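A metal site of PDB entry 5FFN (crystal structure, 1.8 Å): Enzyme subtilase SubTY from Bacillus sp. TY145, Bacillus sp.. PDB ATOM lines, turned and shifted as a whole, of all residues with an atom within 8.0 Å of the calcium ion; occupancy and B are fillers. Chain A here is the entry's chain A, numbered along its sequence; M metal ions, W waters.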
ATOM      1  N   THR A 201       7.940   4.413 -10.685  1.00  0.00           N
ATOM      2  CA  THR A 201       8.377   5.717 -11.140  1.00  0.00           C
ATOM      3  C   THR A 201       9.153   6.421 -10.035  1.00  0.00           C
ATOM      4  O   THR A 201       9.172   5.958  -8.904  1.00  0.00           O
ATOM      5  CB  THR A 201       7.138   6.635 -11.550  1.00  0.00           C
ATOM      6  OG1 THR A 201       6.450   7.137 -10.389  1.00  0.00           O
ATOM      7  CG2 THR A 201       6.151   5.895 -12.391  1.00  0.00           C
ATOM      8  N   VAL A 204       7.391  11.496  -5.587  1.00  0.00           N
ATOM      9  CA  VAL A 204       7.248  12.839  -5.066  1.00  0.00           C
ATOM     10  C   VAL A 204       7.729  12.875  -3.601  1.00  0.00           C
ATOM     11  O   VAL A 204       7.284  12.036  -2.780  1.00  0.00           O
ATOM     12  CB  VAL A 204       5.798  13.334  -5.163  1.00  0.00           C
ATOM     13  CG1 VAL A 204       5.669  14.781  -4.652  1.00  0.00           C
ATOM     14  CG2 VAL A 204       5.317  13.247  -6.614  1.00  0.00           C
ATOM     15  N   TYR A 219      -5.968  17.218 -16.873  1.00  0.00           N
ATOM     16  CA  TYR A 219      -4.888  17.737 -17.720  1.00  0.00           C
ATOM     17  C   TYR A 219      -5.189  19.173 -18.243  1.00  0.00           C
ATOM     18  O   TYR A 219      -4.750  19.548 -19.331  1.00  0.00           O
ATOM     19  CB  TYR A 219      -4.589  16.777 -18.875  1.00  0.00           C
ATOM     20  CG  TYR A 219      -3.892  15.498 -18.462  1.00  0.00           C
ATOM     21  CD1 TYR A 219      -2.609  15.514 -17.964  1.00  0.00           C
ATOM     22  CD2 TYR A 219      -4.527  14.280 -18.592  1.00  0.00           C
ATOM     23  CE1 TYR A 219      -1.956  14.347 -17.584  1.00  0.00           C
ATOM     24  CE2 TYR A 219      -3.894  13.113 -18.244  1.00  0.00           C
ATOM     25  CZ  TYR A 219      -2.628  13.141 -17.735  1.00  0.00           C
ATOM     26  OH  TYR A 219      -2.044  11.936 -17.448  1.00  0.00           O
ATOM     27  N   SER A 229       6.670  17.835 -12.340  1.00  0.00           N
ATOM     28  CA  SER A 229       7.552  17.431 -11.277  1.00  0.00           C
ATOM     29  C   SER A 229       8.989  17.355 -11.799  1.00  0.00           C
ATOM     30  O   SER A 229       9.218  17.090 -13.002  1.00  0.00           O
ATOM     31  CB  SER A 229       7.158  16.057 -10.781  1.00  0.00           C
ATOM     32  OG  SER A 229       5.852  16.065 -10.259  1.00  0.00           O
ATOM     33  N   ALA A 284       5.748  15.955 -19.993  1.00  0.00           N
ATOM     34  CA  ALA A 284       5.442  15.490 -18.630  1.00  0.00           C
ATOM     35  C   ALA A 284       4.642  14.192 -18.695  1.00  0.00           C
ATOM     36  O   ALA A 284       4.867  13.240 -17.944  1.00  0.00           O
ATOM     37  CB  ALA A 284       4.669  16.582 -17.839  1.00  0.00           C
ATOM     38  N   TYR A 287       6.169  10.756 -18.979  1.00  0.00           N
ATOM     39  CA  TYR A 287       6.632  10.185 -17.715  1.00  0.00           C
ATOM     40  C   TYR A 287       5.640  10.484 -16.602  1.00  0.00           C
ATOM     41  O   TYR A 287       5.866  11.330 -15.737  1.00  0.00           O
ATOM     42  CB  TYR A 287       8.050  10.651 -17.405  1.00  0.00           C
ATOM     43  CG  TYR A 287       9.022  10.185 -18.448  1.00  0.00           C
ATOM     44  CD1 TYR A 287       9.462   8.874 -18.470  1.00  0.00           C
ATOM     45  CD2 TYR A 287       9.412  11.025 -19.518  1.00  0.00           C
ATOM     46  CE1 TYR A 287      10.294   8.408 -19.424  1.00  0.00           C
ATOM     47  CE2 TYR A 287      10.273  10.546 -20.492  1.00  0.00           C
ATOM     48  CZ  TYR A 287      10.710   9.230 -20.434  1.00  0.00           C
ATOM     49  OH  TYR A 287      11.554   8.700 -21.362  1.00  0.00           O
ATOM     50  N   ASP A 288       4.510   9.777 -16.658  1.00  0.00           N
ATOM     51  CA  ASP A 288       3.514   9.805 -15.611  1.00  0.00           C
ATOM     52  C   ASP A 288       4.191   9.451 -14.270  1.00  0.00           C
ATOM     53  O   ASP A 288       4.969   8.519 -14.214  1.00  0.00           O
ATOM     54  CB  ASP A 288       2.429   8.776 -15.938  1.00  0.00           C
ATOM     55  CG  ASP A 288       1.189   8.865 -15.032  1.00  0.00           C
ATOM     56  OD1 ASP A 288       1.052   9.834 -14.224  1.00  0.00           O
ATOM     57  OD2 ASP A 288       0.308   7.968 -15.143  1.00  0.00           O
ATOM     58  N   ILE A 289       3.971  10.240 -13.219  1.00  0.00           N
ATOM     59  CA  ILE A 289       4.528   9.902 -11.874  1.00  0.00           C
ATOM     60  C   ILE A 289       3.438   9.268 -11.032  1.00  0.00           C
ATOM     61  O   ILE A 289       2.294   9.769 -10.943  1.00  0.00           O
ATOM     62  CB  ILE A 289       5.167  11.163 -11.208  1.00  0.00           C
ATOM     63  CG1 ILE A 289       6.346  11.684 -12.040  1.00  0.00           C
ATOM     64  CG2 ILE A 289       5.531  10.938  -9.732  1.00  0.00           C
ATOM     65  CD1 ILE A 289       7.698  10.835 -11.959  1.00  0.00           C
ATOM     66  N   LYS A 290       3.770   8.131 -10.407  1.00  0.00           N
ATOM     67  CA  LYS A 290       2.813   7.341  -9.653  1.00  0.00           C
ATOM     68  C   LYS A 290       3.264   7.089  -8.197  1.00  0.00           C
ATOM     69  O   LYS A 290       2.533   6.440  -7.435  1.00  0.00           O
ATOM     70  CB  LYS A 290       2.649   5.997 -10.352  1.00  0.00           C
ATOM     71  CG  LYS A 290       1.965   6.143 -11.743  1.00  0.00           C
ATOM     72  CD  LYS A 290       1.404   4.810 -12.216  1.00  0.00           C
ATOM     73  CE  LYS A 290       2.325   4.139 -13.169  1.00  0.00           C
ATOM     74  NZ  LYS A 290       1.958   2.667 -13.403  1.00  0.00           N
ATOM     75  N   GLY A 291       4.444   7.576  -7.856  1.00  0.00           N
ATOM     76  CA  GLY A 291       5.025   7.394  -6.544  1.00  0.00           C
ATOM     77  C   GLY A 291       4.865   8.607  -5.658  1.00  0.00           C
ATOM     78  O   GLY A 291       5.042   9.764  -6.128  1.00  0.00           O
ATOM     79  N   GLY A 294      -0.533  10.714  -2.569  1.00  0.00           N
ATOM     80  CA  GLY A 294      -1.446  11.385  -3.524  1.00  0.00           C
ATOM     81  C   GLY A 294      -1.124  11.254  -5.008  1.00  0.00           C
ATOM     82  O   GLY A 294      -1.892  11.753  -5.879  1.00  0.00           O
ATOM     83  N   ALA A 295      -0.027  10.597  -5.340  1.00  0.00           N
ATOM     84  CA  ALA A 295       0.359  10.389  -6.709  1.00  0.00           C
ATOM     85  C   ALA A 295      -0.409   9.191  -7.216  1.00  0.00           C
ATOM     86  O   ALA A 295      -0.833   8.323  -6.443  1.00  0.00           O
ATOM     87  CB  ALA A 295       1.917  10.194  -6.874  1.00  0.00           C
ATOM     88  N   GLY A 296      -0.638   9.141  -8.519  1.00  0.00           N
ATOM     89  CA  GLY A 296      -1.349   7.987  -9.082  1.00  0.00           C
ATOM     90  C   GLY A 296      -1.338   8.059 -10.591  1.00  0.00           C
ATOM     91  O   GLY A 296      -0.693   8.914 -11.173  1.00  0.00           O
ATOM     92  N   THR A 297      -2.022   7.128 -11.238  1.00  0.00           N
ATOM     93  CA  THR A 297      -2.026   7.115 -12.686  1.00  0.00           C
ATOM     94  C   THR A 297      -2.696   8.380 -13.236  1.00  0.00           C
ATOM     95  O   THR A 297      -3.771   8.748 -12.794  1.00  0.00           O
ATOM     96  CB  THR A 297      -2.780   5.864 -13.174  1.00  0.00           C
ATOM     97  OG1 THR A 297      -2.109   4.703 -12.639  1.00  0.00           O
ATOM     98  CG2 THR A 297      -2.800   5.822 -14.670  1.00  0.00           C
ATOM     99  N   GLY A 298      -2.054   9.048 -14.181  1.00  0.00           N
ATOM    100  CA  GLY A 298      -2.613  10.240 -14.785  1.00  0.00           C
ATOM    101  C   GLY A 298      -2.259  11.513 -14.041  1.00  0.00           C
ATOM    102  O   GLY A 298      -1.337  11.557 -13.217  1.00  0.00           O
ATOM    103  N   ASP A 299      -2.987  12.557 -14.362  1.00  0.00           N
ATOM    104  CA  ASP A 299      -2.789  13.875 -13.750  1.00  0.00           C
ATOM    105  C   ASP A 299      -3.206  13.802 -12.317  1.00  0.00           C
ATOM    106  O   ASP A 299      -4.340  13.386 -12.016  1.00  0.00           O
ATOM    107  CB  ASP A 299      -3.602  14.868 -14.559  1.00  0.00           C
ATOM    108  CG  ASP A 299      -3.651  16.271 -13.979  1.00  0.00           C
ATOM    109  OD1 ASP A 299      -2.678  16.670 -13.346  1.00  0.00           O
ATOM    110  OD2 ASP A 299      -4.702  16.946 -14.214  1.00  0.00           O
ATOM    111  N   ASP A 300      -2.306  14.113 -11.394  1.00  0.00           N
ATOM    112  CA  ASP A 300      -2.637  13.995  -9.980  1.00  0.00           C
ATOM    113  C   ASP A 300      -2.126  15.222  -9.221  1.00  0.00           C
ATOM    114  O   ASP A 300      -1.308  16.030  -9.719  1.00  0.00           O
ATOM    115  CB  ASP A 300      -2.108  12.660  -9.392  1.00  0.00           C
ATOM    116  CG  ASP A 300      -0.604  12.608  -9.320  1.00  0.00           C
ATOM    117  OD1 ASP A 300      -0.023  13.381  -8.556  1.00  0.00           O
ATOM    118  OD2 ASP A 300       0.009  11.719  -9.938  1.00  0.00           O
ATOM    119  N   TYR A 301      -2.629  15.370  -8.008  1.00  0.00           N
ATOM    120  CA  TYR A 301      -2.353  16.571  -7.233  1.00  0.00           C
ATOM    121  C   TYR A 301      -1.006  16.511  -6.453  1.00  0.00           C
ATOM    122  O   TYR A 301      -0.637  17.488  -5.815  1.00  0.00           O
ATOM    123  CB  TYR A 301      -3.521  16.876  -6.291  1.00  0.00           C
ATOM    124  CG  TYR A 301      -3.858  15.780  -5.307  1.00  0.00           C
ATOM    125  CD1 TYR A 301      -3.150  15.638  -4.132  1.00  0.00           C
ATOM    126  CD2 TYR A 301      -4.842  14.835  -5.591  1.00  0.00           C
ATOM    127  CE1 TYR A 301      -3.445  14.580  -3.230  1.00  0.00           C
ATOM    128  CE2 TYR A 301      -5.162  13.812  -4.698  1.00  0.00           C
ATOM    129  CZ  TYR A 301      -4.464  13.688  -3.513  1.00  0.00           C
ATOM    130  OH  TYR A 301      -4.774  12.653  -2.607  1.00  0.00           O
ATOM    131  N   ALA A 302      -0.242  15.400  -6.560  1.00  0.00           N
ATOM    132  CA  ALA A 302       1.125  15.384  -6.053  1.00  0.00           C
ATOM    133  C   ALA A 302       2.178  15.753  -7.090  1.00  0.00           C
ATOM    134  O   ALA A 302       3.127  16.480  -6.791  1.00  0.00           O
ATOM    135  CB  ALA A 302       1.489  14.004  -5.464  1.00  0.00           C
ATOM    136  N   SER A 303       2.001  15.250  -8.305  1.00  0.00           N
ATOM    137  CA  SER A 303       3.017  15.366  -9.327  1.00  0.00           C
ATOM    138  C   SER A 303       2.541  16.100 -10.603  1.00  0.00           C
ATOM    139  O   SER A 303       3.312  16.273 -11.519  1.00  0.00           O
ATOM    140  CB  SER A 303       3.511  13.981  -9.716  1.00  0.00           C
ATOM    141  OG  SER A 303       2.496  13.214 -10.377  1.00  0.00           O
ATOM    142  N   GLY A 304       1.273  16.484 -10.653  1.00  0.00           N
ATOM    143  CA  GLY A 304       0.717  17.118 -11.824  1.00  0.00           C
ATOM    144  C   GLY A 304       0.715  16.175 -13.015  1.00  0.00           C
ATOM    145  O   GLY A 304       0.339  15.018 -12.898  1.00  0.00           O
ATOM    146  N   PHE A 305       1.099  16.702 -14.170  1.00  0.00           N
ATOM    147  CA  PHE A 305       1.020  15.988 -15.415  1.00  0.00           C
ATOM    148  C   PHE A 305       2.104  14.939 -15.543  1.00  0.00           C
ATOM    149  O   PHE A 305       1.965  14.033 -16.362  1.00  0.00           O
ATOM    150  CB  PHE A 305       1.164  16.928 -16.632  1.00  0.00           C
ATOM    151  CG  PHE A 305       0.013  17.902 -16.866  1.00  0.00           C
ATOM    152  CD1 PHE A 305      -0.937  18.205 -15.887  1.00  0.00           C
ATOM    153  CD2 PHE A 305      -0.053  18.591 -18.081  1.00  0.00           C
ATOM    154  CE1 PHE A 305      -1.972  19.151 -16.118  1.00  0.00           C
ATOM    155  CE2 PHE A 305      -1.079  19.503 -18.321  1.00  0.00           C
ATOM    156  CZ  PHE A 305      -2.024  19.794 -17.357  1.00  0.00           C
ATOM    157  N   GLY A 306       3.148  15.036 -14.724  1.00  0.00           N
ATOM    158  CA  GLY A 306       4.222  14.080 -14.785  1.00  0.00           C
ATOM    159  C   GLY A 306       5.556  14.774 -14.724  1.00  0.00           C
ATOM    160  O   GLY A 306       5.693  15.910 -14.222  1.00  0.00           O
ATOM    161  N   TYR A 307       6.544  14.085 -15.257  1.00  0.00           N
ATOM    162  CA  TYR A 307       7.945  14.493 -15.205  1.00  0.00           C
ATOM    163  C   TYR A 307       8.521  14.763 -16.599  1.00  0.00           C
ATOM    164  O   TYR A 307       8.914  13.830 -17.298  1.00  0.00           O
ATOM    165  CB  TYR A 307       8.727  13.368 -14.498  1.00  0.00           C
ATOM    166  CG  TYR A 307      10.220  13.553 -14.365  1.00  0.00           C
ATOM    167  CD1 TYR A 307      10.854  14.793 -14.561  1.00  0.00           C
ATOM    168  CD2 TYR A 307      11.035  12.449 -13.999  1.00  0.00           C
ATOM    169  CE1 TYR A 307      12.228  14.948 -14.452  1.00  0.00           C
ATOM    170  CE2 TYR A 307      12.407  12.587 -13.840  1.00  0.00           C
ATOM    171  CZ  TYR A 307      13.016  13.862 -14.044  1.00  0.00           C
ATOM    172  OH  TYR A 307      14.372  14.058 -13.946  1.00  0.00           O
HETATM  173 CA    CA M   1       0.455  10.707 -12.082  1.00  0.00          CA
HETATM  174  O   HOH W   1       1.810  12.539 -12.870  1.00  0.00           O
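The backbone NH (N) of Ser 303 sits at hydrogen-bond distance from the side-chain carboxylate (OD1) of Asp 300 (2.8 Å). The backbone carbonyl oxygen (O) of Ser 303 is in hydrogen-bond range of the side-chain hydroxyl (OG) of Ser 229 (2.8 Å). O of Ile 289 sits close to OG of Ser 303 (3.5 Å). The side-chain carboxylate (OD1) of Asp 300 lies within hydrogen-bond range of the backbone NH (N) of Ala 302, at 2.8 Å.
Residues that only touch the calcium ion: Ser 303 (3.7 Å). Of the 24 residues printed, 6 come within 4 Å of the calcium ion.
The calcium ion is bound by O of Gly 298 (2.3 Å), O of Gly 296 (2.3 Å), O of Ile 289 (2.4 Å), OD1 of Asp 288 (2.4 Å), water W1 (2.4 Å) and OD2 of Asp 300 (2.4 Å).
Water W1 lies within hydrogen-bond range of OG of Ser 303, O of Gly 304, N of Ile 289 and N of Gly 306.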
